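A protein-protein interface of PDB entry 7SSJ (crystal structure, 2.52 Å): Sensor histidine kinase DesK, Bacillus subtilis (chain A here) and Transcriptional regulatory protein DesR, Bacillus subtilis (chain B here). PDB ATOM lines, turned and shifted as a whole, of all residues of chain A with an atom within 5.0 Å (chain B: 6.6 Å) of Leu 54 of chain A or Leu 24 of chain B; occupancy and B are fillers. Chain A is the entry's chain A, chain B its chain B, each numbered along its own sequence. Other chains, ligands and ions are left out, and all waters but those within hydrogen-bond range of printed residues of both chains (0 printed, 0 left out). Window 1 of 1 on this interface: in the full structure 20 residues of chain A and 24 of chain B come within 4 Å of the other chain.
OG of Ser 50 of chain A touches CB of Asp 107 of chain B (3.8 Å).
CD1 of Leu 54 of chain A touches CD2 of Leu 17 of chain B (3.5 Å).
Leu 54 of chain A touches Leu 24 of chain B (O to CD1, 3.6 Å).
Lys 106 of chain B touches Leu 54 of chain A.
Lys 55 of chain A touches Ala 20 of chain B.
CD2 of Leu 24 of chain B touches OD1 of Asp 57 of chain A, 3.9 Å away.
Pro 109 of chain B touches Asp 57 of chain A.
CD2 of Leu 24 of chain B touches N of Leu 58 of chain A, at 3.6 Å.
Leu 58 of chain A touches Leu 27 of chain B (CD1 to CD2, 3.8 Å).
Leu 27 of chain B touches Lys 61 of chain A (CD2 to CB, 3.9 Å).
Of the 10 printed residues of chain A, 7 touch a printed residue of chain B.
Hydrophobic or aromatic side chains of chain B that line the printed part of chain A: Leu 17, Ala 20, Leu 21, Leu 24 and Leu 27.
Leu 54 of chain A touches just these residues of chain B: Leu 17, Leu 21, Leu 24 and Lys 106.
Glu 12 of chain B touches none of the printed residues of chain A.
Of the printed residues of chain A, Ser 23 of chain B touches Leu 58.
Of chain A, only Leu 54, Asp 57 and Leu 58 come within 4 Å of Leu 24 of chain B.
Printed residues of chain A within 4 Å of Asp 107 of chain B: Ser 50.
NZ of Lys 106 of chain B is in salt-bridge range of OE1 of Glu 12 of chain B (2.7 Å).
O of Gly 19 of chain B lies within hydrogen-bond range of OG of Ser 23 of chain B (3.3 Å).
OD1 of Asp 57 of chain A lies within hydrogen-bond range of OG of Ser 110 of chain B.
NZ of Lys 61 of chain A is in hydrogen-bond range of OG of Ser 110 of chain B.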
ATOM      1  N   SER A  50      -6.070  32.260  26.691  1.00  0.00           N
ATOM      2  CA  SER A  50      -6.261  31.310  25.598  1.00  0.00           C
ATOM      3  C   SER A  50      -4.898  31.002  24.957  1.00  0.00           C
ATOM      4  O   SER A  50      -4.593  29.858  24.661  1.00  0.00           O
ATOM      5  CB  SER A  50      -7.208  31.884  24.545  1.00  0.00           C
ATOM      6  OG  SER A  50      -8.522  32.069  25.042  1.00  0.00           O
ATOM      7  N   LEU A  51      -4.068  32.018  24.778  1.00  0.00           N
ATOM      8  CA  LEU A  51      -2.738  31.856  24.212  1.00  0.00           C
ATOM      9  C   LEU A  51      -1.846  30.994  25.111  1.00  0.00           C
ATOM     10  O   LEU A  51      -1.231  30.057  24.620  1.00  0.00           O
ATOM     11  CB  LEU A  51      -2.144  33.227  23.970  1.00  0.00           C
ATOM     12  CG  LEU A  51      -0.694  33.282  23.554  1.00  0.00           C
ATOM     13  CD1 LEU A  51      -0.472  32.581  22.202  1.00  0.00           C
ATOM     14  CD2 LEU A  51      -0.208  34.718  23.595  1.00  0.00           C
ATOM     15  N   ILE A  52      -1.812  31.243  26.414  1.00  0.00           N
ATOM     16  CA  ILE A  52      -1.037  30.422  27.366  1.00  0.00           C
ATOM     17  C   ILE A  52      -1.407  28.972  27.288  1.00  0.00           C
ATOM     18  O   ILE A  52      -0.517  28.145  27.208  1.00  0.00           O
ATOM     19  CB  ILE A  52      -1.182  30.956  28.810  1.00  0.00           C
ATOM     20  CG1 ILE A  52      -0.541  32.375  28.914  1.00  0.00           C
ATOM     21  CG2 ILE A  52      -0.630  29.985  29.844  1.00  0.00           C
ATOM     22  CD1 ILE A  52      -0.843  33.106  30.147  1.00  0.00           C
ATOM     23  N   GLY A  53      -2.704  28.675  27.246  1.00  0.00           N
ATOM     24  CA  GLY A  53      -3.202  27.311  27.134  1.00  0.00           C
ATOM     25  C   GLY A  53      -2.782  26.629  25.848  1.00  0.00           C
ATOM     26  O   GLY A  53      -2.216  25.522  25.868  1.00  0.00           O
ATOM     27  N   LEU A  54      -3.011  27.305  24.720  1.00  0.00           N
ATOM     28  CA  LEU A  54      -2.631  26.755  23.417  1.00  0.00           C
ATOM     29  C   LEU A  54      -1.129  26.567  23.249  1.00  0.00           C
ATOM     30  O   LEU A  54      -0.700  25.571  22.659  1.00  0.00           O
ATOM     31  CB  LEU A  54      -3.223  27.582  22.264  1.00  0.00           C
ATOM     32  CG  LEU A  54      -4.773  27.643  22.201  1.00  0.00           C
ATOM     33  CD1 LEU A  54      -5.205  28.248  20.915  1.00  0.00           C
ATOM     34  CD2 LEU A  54      -5.435  26.256  22.323  1.00  0.00           C
ATOM     35  N   LYS A  55      -0.326  27.516  23.750  1.00  0.00           N
ATOM     36  CA  LYS A  55       1.138  27.418  23.642  1.00  0.00           C
ATOM     37  C   LYS A  55       1.683  26.351  24.570  1.00  0.00           C
ATOM     38  O   LYS A  55       2.686  25.748  24.234  1.00  0.00           O
ATOM     39  CB  LYS A  55       1.840  28.767  23.830  1.00  0.00           C
ATOM     40  CG  LYS A  55       2.184  29.486  22.531  1.00  0.00           C
ATOM     41  CD  LYS A  55       2.912  30.839  22.800  1.00  0.00           C
ATOM     42  CE  LYS A  55       3.967  31.220  21.797  1.00  0.00           C
ATOM     43  NZ  LYS A  55       3.424  31.500  20.431  1.00  0.00           N
ATOM     44  N   SER A  56       1.003  26.071  25.704  1.00  0.00           N
ATOM     45  CA  SER A  56       1.401  24.984  26.602  1.00  0.00           C
ATOM     46  C   SER A  56       1.098  23.642  25.941  1.00  0.00           C
ATOM     47  O   SER A  56       1.921  22.738  25.980  1.00  0.00           O
ATOM     48  CB  SER A  56       0.648  25.071  27.918  1.00  0.00           C
ATOM     49  OG  SER A  56       1.111  26.232  28.569  1.00  0.00           O
ATOM     50  N   ASP A  57      -0.082  23.522  25.311  1.00  0.00           N
ATOM     51  CA  ASP A  57      -0.513  22.351  24.560  1.00  0.00           C
ATOM     52  C   ASP A  57       0.527  22.056  23.460  1.00  0.00           C
ATOM     53  O   ASP A  57       1.007  20.946  23.373  1.00  0.00           O
ATOM     54  CB  ASP A  57      -1.891  22.655  23.952  1.00  0.00           C
ATOM     55  CG  ASP A  57      -2.712  21.472  23.501  1.00  0.00           C
ATOM     56  OD1 ASP A  57      -2.119  20.477  23.047  1.00  0.00           O
ATOM     57  OD2 ASP A  57      -3.953  21.549  23.578  1.00  0.00           O
ATOM     58  N   LEU A  58       0.967  23.069  22.715  1.00  0.00           N
ATOM     59  CA  LEU A  58       1.989  22.920  21.690  1.00  0.00           C
ATOM     60  C   LEU A  58       3.344  22.545  22.264  1.00  0.00           C
ATOM     61  O   LEU A  58       3.941  21.600  21.776  1.00  0.00           O
ATOM     62  CB  LEU A  58       2.100  24.212  20.890  1.00  0.00           C
ATOM     63  CG  LEU A  58       3.143  24.270  19.806  1.00  0.00           C
ATOM     64  CD1 LEU A  58       2.966  23.107  18.782  1.00  0.00           C
ATOM     65  CD2 LEU A  58       3.138  25.654  19.163  1.00  0.00           C
ATOM     66  N   LYS A  61       3.332  18.916  23.215  1.00  0.00           N
ATOM     67  CA  LYS A  61       3.432  18.074  22.033  1.00  0.00           C
ATOM     68  C   LYS A  61       4.831  18.080  21.424  1.00  0.00           C
ATOM     69  O   LYS A  61       5.216  17.100  20.802  1.00  0.00           O
ATOM     70  CB  LYS A  61       2.358  18.444  21.002  1.00  0.00           C
ATOM     71  CG  LYS A  61       0.973  18.296  21.585  1.00  0.00           C
ATOM     72  CD  LYS A  61      -0.120  18.135  20.562  1.00  0.00           C
ATOM     73  CE  LYS A  61      -1.357  17.643  21.300  1.00  0.00           C
ATOM     74  NZ  LYS A  61      -2.561  17.457  20.422  1.00  0.00           N
ATOM     75  N   GLU B  12      -7.292  34.496  12.532  1.00  0.00           N
ATOM     76  CA  GLU B  12      -7.180  34.916  13.916  1.00  0.00           C
ATOM     77  C   GLU B  12      -6.442  36.228  13.926  1.00  0.00           C
ATOM     78  O   GLU B  12      -5.359  36.291  13.347  1.00  0.00           O
ATOM     79  CB  GLU B  12      -6.316  33.918  14.694  1.00  0.00           C
ATOM     80  CG  GLU B  12      -6.942  33.446  15.976  1.00  0.00           C
ATOM     81  CD  GLU B  12      -6.975  34.407  17.145  1.00  0.00           C
ATOM     82  OE1 GLU B  12      -6.973  33.928  18.294  1.00  0.00           O
ATOM     83  OE2 GLU B  12      -7.023  35.634  16.934  1.00  0.00           O
ATOM     84  N   LEU B  17      -1.336  33.688  18.790  1.00  0.00           N
ATOM     85  CA  LEU B  17      -2.380  32.675  18.793  1.00  0.00           C
ATOM     86  C   LEU B  17      -2.517  32.029  17.452  1.00  0.00           C
ATOM     87  O   LEU B  17      -2.691  30.815  17.364  1.00  0.00           O
ATOM     88  CB  LEU B  17      -3.714  33.320  19.227  1.00  0.00           C
ATOM     89  CG  LEU B  17      -4.451  32.608  20.347  1.00  0.00           C
ATOM     90  CD1 LEU B  17      -5.239  33.552  21.176  1.00  0.00           C
ATOM     91  CD2 LEU B  17      -5.310  31.522  19.792  1.00  0.00           C
ATOM     92  N   GLY B  19      -0.188  31.706  15.288  1.00  0.00           N
ATOM     93  CA  GLY B  19       0.999  30.881  15.182  1.00  0.00           C
ATOM     94  C   GLY B  19       0.805  29.532  15.837  1.00  0.00           C
ATOM     95  O   GLY B  19       0.871  28.507  15.155  1.00  0.00           O
ATOM     96  N   ALA B  20       0.511  29.520  17.154  1.00  0.00           N
ATOM     97  CA  ALA B  20       0.262  28.296  17.915  1.00  0.00           C
ATOM     98  C   ALA B  20      -0.843  27.413  17.293  1.00  0.00           C
ATOM     99  O   ALA B  20      -0.689  26.205  17.232  1.00  0.00           O
ATOM    100  CB  ALA B  20      -0.079  28.644  19.351  1.00  0.00           C
ATOM    101  N   LEU B  21      -1.949  28.008  16.820  1.00  0.00           N
ATOM    102  CA  LEU B  21      -3.036  27.248  16.221  1.00  0.00           C
ATOM    103  C   LEU B  21      -2.576  26.569  14.969  1.00  0.00           C
ATOM    104  O   LEU B  21      -2.926  25.417  14.747  1.00  0.00           O
ATOM    105  CB  LEU B  21      -4.247  28.145  15.910  1.00  0.00           C
ATOM    106  CG  LEU B  21      -5.205  28.443  17.065  1.00  0.00           C
ATOM    107  CD1 LEU B  21      -6.157  29.568  16.698  1.00  0.00           C
ATOM    108  CD2 LEU B  21      -5.955  27.179  17.517  1.00  0.00           C
ATOM    109  N   GLY B  22      -1.804  27.281  14.151  1.00  0.00           N
ATOM    110  CA  GLY B  22      -1.258  26.761  12.904  1.00  0.00           C
ATOM    111  C   GLY B  22      -0.298  25.612  13.141  1.00  0.00           C
ATOM    112  O   GLY B  22      -0.411  24.589  12.478  1.00  0.00           O
ATOM    113  N   SER B  23       0.594  25.743  14.149  1.00  0.00           N
ATOM    114  CA  SER B  23       1.559  24.724  14.528  1.00  0.00           C
ATOM    115  C   SER B  23       0.877  23.492  15.079  1.00  0.00           C
ATOM    116  O   SER B  23       1.247  22.377  14.719  1.00  0.00           O
ATOM    117  CB  SER B  23       2.540  25.273  15.548  1.00  0.00           C
ATOM    118  OG  SER B  23       3.351  26.293  14.987  1.00  0.00           O
ATOM    119  N   LEU B  24      -0.154  23.675  15.922  1.00  0.00           N
ATOM    120  CA  LEU B  24      -0.911  22.577  16.501  1.00  0.00           C
ATOM    121  C   LEU B  24      -1.655  21.780  15.441  1.00  0.00           C
ATOM    122  O   LEU B  24      -1.606  20.548  15.478  1.00  0.00           O
ATOM    123  CB  LEU B  24      -1.891  23.095  17.556  1.00  0.00           C
ATOM    124  CG  LEU B  24      -1.280  23.513  18.877  1.00  0.00           C
ATOM    125  CD1 LEU B  24      -2.147  24.530  19.543  1.00  0.00           C
ATOM    126  CD2 LEU B  24      -1.099  22.352  19.795  1.00  0.00           C
ATOM    127  N   LEU B  25      -2.357  22.452  14.517  1.00  0.00           N
ATOM    128  CA  LEU B  25      -3.104  21.720  13.500  1.00  0.00           C
ATOM    129  C   LEU B  25      -2.202  21.011  12.502  1.00  0.00           C
ATOM    130  O   LEU B  25      -2.538  19.928  12.035  1.00  0.00           O
ATOM    131  CB  LEU B  25      -4.101  22.616  12.799  1.00  0.00           C
ATOM    132  CG  LEU B  25      -5.312  23.030  13.633  1.00  0.00           C
ATOM    133  CD1 LEU B  25      -6.215  23.975  12.840  1.00  0.00           C
ATOM    134  CD2 LEU B  25      -6.117  21.802  14.105  1.00  0.00           C
ATOM    135  N   ASN B  26      -1.054  21.617  12.180  1.00  0.00           N
ATOM    136  CA  ASN B  26      -0.075  21.075  11.250  1.00  0.00           C
ATOM    137  C   ASN B  26       0.507  19.745  11.771  1.00  0.00           C
ATOM    138  O   ASN B  26       0.693  18.788  10.996  1.00  0.00           O
ATOM    139  CB  ASN B  26       1.015  22.088  11.029  1.00  0.00           C
ATOM    140  CG  ASN B  26       0.810  22.910   9.787  1.00  0.00           C
ATOM    141  OD1 ASN B  26       0.144  22.496   8.844  1.00  0.00           O
ATOM    142  ND2 ASN B  26       1.392  24.097   9.756  1.00  0.00           N
ATOM    143  N   LEU B  27       0.717  19.667  13.094  1.00  0.00           N
ATOM    144  CA  LEU B  27       1.197  18.489  13.815  1.00  0.00           C
ATOM    145  C   LEU B  27       0.287  17.258  13.623  1.00  0.00           C
ATOM    146  O   LEU B  27       0.717  16.148  13.908  1.00  0.00           O
ATOM    147  CB  LEU B  27       1.266  18.845  15.304  1.00  0.00           C
ATOM    148  CG  LEU B  27       2.598  18.838  16.042  1.00  0.00           C
ATOM    149  CD1 LEU B  27       3.721  19.390  15.230  1.00  0.00           C
ATOM    150  CD2 LEU B  27       2.476  19.624  17.321  1.00  0.00           C
ATOM    151  N   GLU B  28      -0.943  17.431  13.138  1.00  0.00           N
ATOM    152  CA  GLU B  28      -1.835  16.307  12.892  1.00  0.00           C
ATOM    153  C   GLU B  28      -1.495  15.687  11.561  1.00  0.00           C
ATOM    154  O   GLU B  28      -1.280  16.405  10.576  1.00  0.00           O
ATOM    155  CB  GLU B  28      -3.288  16.744  12.973  1.00  0.00           C
ATOM    156  CG  GLU B  28      -3.641  17.182  14.380  1.00  0.00           C
ATOM    157  CD  GLU B  28      -4.006  16.048  15.315  1.00  0.00           C
ATOM    158  OE1 GLU B  28      -4.370  14.955  14.816  1.00  0.00           O
ATOM    159  OE2 GLU B  28      -3.956  16.260  16.549  1.00  0.00           O
ATOM    160  N   VAL B  33      -2.240  23.127   7.420  1.00  0.00           N
ATOM    161  CA  VAL B  33      -2.682  24.510   7.286  1.00  0.00           C
ATOM    162  C   VAL B  33      -2.251  25.083   5.914  1.00  0.00           C
ATOM    163  O   VAL B  33      -1.060  25.185   5.620  1.00  0.00           O
ATOM    164  CB  VAL B  33      -2.192  25.383   8.447  1.00  0.00           C
ATOM    165  CG1 VAL B  33      -2.592  26.829   8.228  1.00  0.00           C
ATOM    166  CG2 VAL B  33      -2.730  24.866   9.770  1.00  0.00           C
ATOM    167  N   LEU B  83     -14.510  29.983  16.370  1.00  0.00           N
ATOM    168  CA  LEU B  83     -13.858  29.903  17.657  1.00  0.00           C
ATOM    169  C   LEU B  83     -14.012  31.253  18.272  1.00  0.00           C
ATOM    170  O   LEU B  83     -13.915  32.247  17.559  1.00  0.00           O
ATOM    171  CB  LEU B  83     -12.351  29.624  17.487  1.00  0.00           C
ATOM    172  CG  LEU B  83     -11.878  28.265  16.915  1.00  0.00           C
ATOM    173  CD1 LEU B  83     -10.375  28.161  17.019  1.00  0.00           C
ATOM    174  CD2 LEU B  83     -12.454  27.127  17.688  1.00  0.00           C
ATOM    175  N   LYS B 106     -12.097  28.920  22.086  1.00  0.00           N
ATOM    176  CA  LYS B 106     -10.728  28.983  21.582  1.00  0.00           C
ATOM    177  C   LYS B 106      -9.701  28.166  22.363  1.00  0.00           C
ATOM    178  O   LYS B 106      -8.831  27.521  21.746  1.00  0.00           O
ATOM    179  CB  LYS B 106     -10.261  30.434  21.500  1.00  0.00           C
ATOM    180  CG  LYS B 106      -9.184  30.615  20.455  1.00  0.00           C
ATOM    181  CD  LYS B 106      -9.000  32.064  20.197  1.00  0.00           C
ATOM    182  CE  LYS B 106      -9.993  32.506  19.183  1.00  0.00           C
ATOM    183  NZ  LYS B 106      -9.666  33.876  18.793  1.00  0.00           N
ATOM    184  N   ASP B 107      -9.802  28.210  23.706  1.00  0.00           N
ATOM    185  CA  ASP B 107      -8.884  27.571  24.620  1.00  0.00           C
ATOM    186  C   ASP B 107      -9.188  26.087  24.908  1.00  0.00           C
ATOM    187  O   ASP B 107      -8.514  25.479  25.754  1.00  0.00           O
ATOM    188  CB  ASP B 107      -8.793  28.372  25.916  1.00  0.00           C
ATOM    189  CG  ASP B 107     -10.062  28.344  26.748  1.00  0.00           C
ATOM    190  OD1 ASP B 107     -11.168  28.210  26.159  1.00  0.00           O
ATOM    191  OD2 ASP B 107      -9.955  28.457  27.979  1.00  0.00           O
ATOM    192  N   SER B 108     -10.160  25.493  24.203  1.00  0.00           N
ATOM    193  CA  SER B 108     -10.439  24.076  24.359  1.00  0.00           C
ATOM    194  C   SER B 108      -9.234  23.284  23.801  1.00  0.00           C
ATOM    195  O   SER B 108      -8.584  23.734  22.840  1.00  0.00           O
ATOM    196  CB  SER B 108     -11.743  23.693  23.652  1.00  0.00           C
ATOM    197  OG  SER B 108     -11.678  23.895  22.250  1.00  0.00           O
ATOM    198  N   PRO B 109      -8.883  22.150  24.444  1.00  0.00           N
ATOM    199  CA  PRO B 109      -7.721  21.363  23.994  1.00  0.00           C
ATOM    200  C   PRO B 109      -7.621  21.118  22.490  1.00  0.00           C
ATOM    201  O   PRO B 109      -8.634  21.083  21.778  1.00  0.00           O
ATOM    202  CB  PRO B 109      -7.899  20.042  24.746  1.00  0.00           C
ATOM    203  CG  PRO B 109      -8.608  20.414  25.983  1.00  0.00           C
ATOM    204  CD  PRO B 109      -9.536  21.535  25.616  1.00  0.00           C
ATOM    205  N   SER B 110      -6.388  20.959  22.011  1.00  0.00           N
ATOM    206  CA  SER B 110      -6.120  20.739  20.594  1.00  0.00           C
ATOM    207  C   SER B 110      -6.717  19.417  20.103  1.00  0.00           C
ATOM    208  O   SER B 110      -7.141  19.321  18.951  1.00  0.00           O
ATOM    209  CB  SER B 110      -4.618  20.754  20.336  1.00  0.00           C
ATOM    210  OG  SER B 110      -3.985  19.684  21.029  1.00  0.00           O
ATOM    211  N   LEU B 113     -10.337  20.089  19.291  1.00  0.00           N
ATOM    212  CA  LEU B 113     -10.395  20.856  18.055  1.00  0.00           C
ATOM    213  C   LEU B 113     -10.121  19.982  16.849  1.00  0.00           C
ATOM    214  O   LEU B 113     -10.846  20.041  15.868  1.00  0.00           O
ATOM    215  CB  LEU B 113      -9.391  22.014  18.101  1.00  0.00           C
ATOM    216  CG  LEU B 113      -9.432  23.008  16.881  1.00  0.00           C
ATOM    217  CD1 LEU B 113     -10.900  23.497  16.560  1.00  0.00           C
ATOM    218  CD2 LEU B 113      -8.451  24.179  17.075  1.00  0.00           C
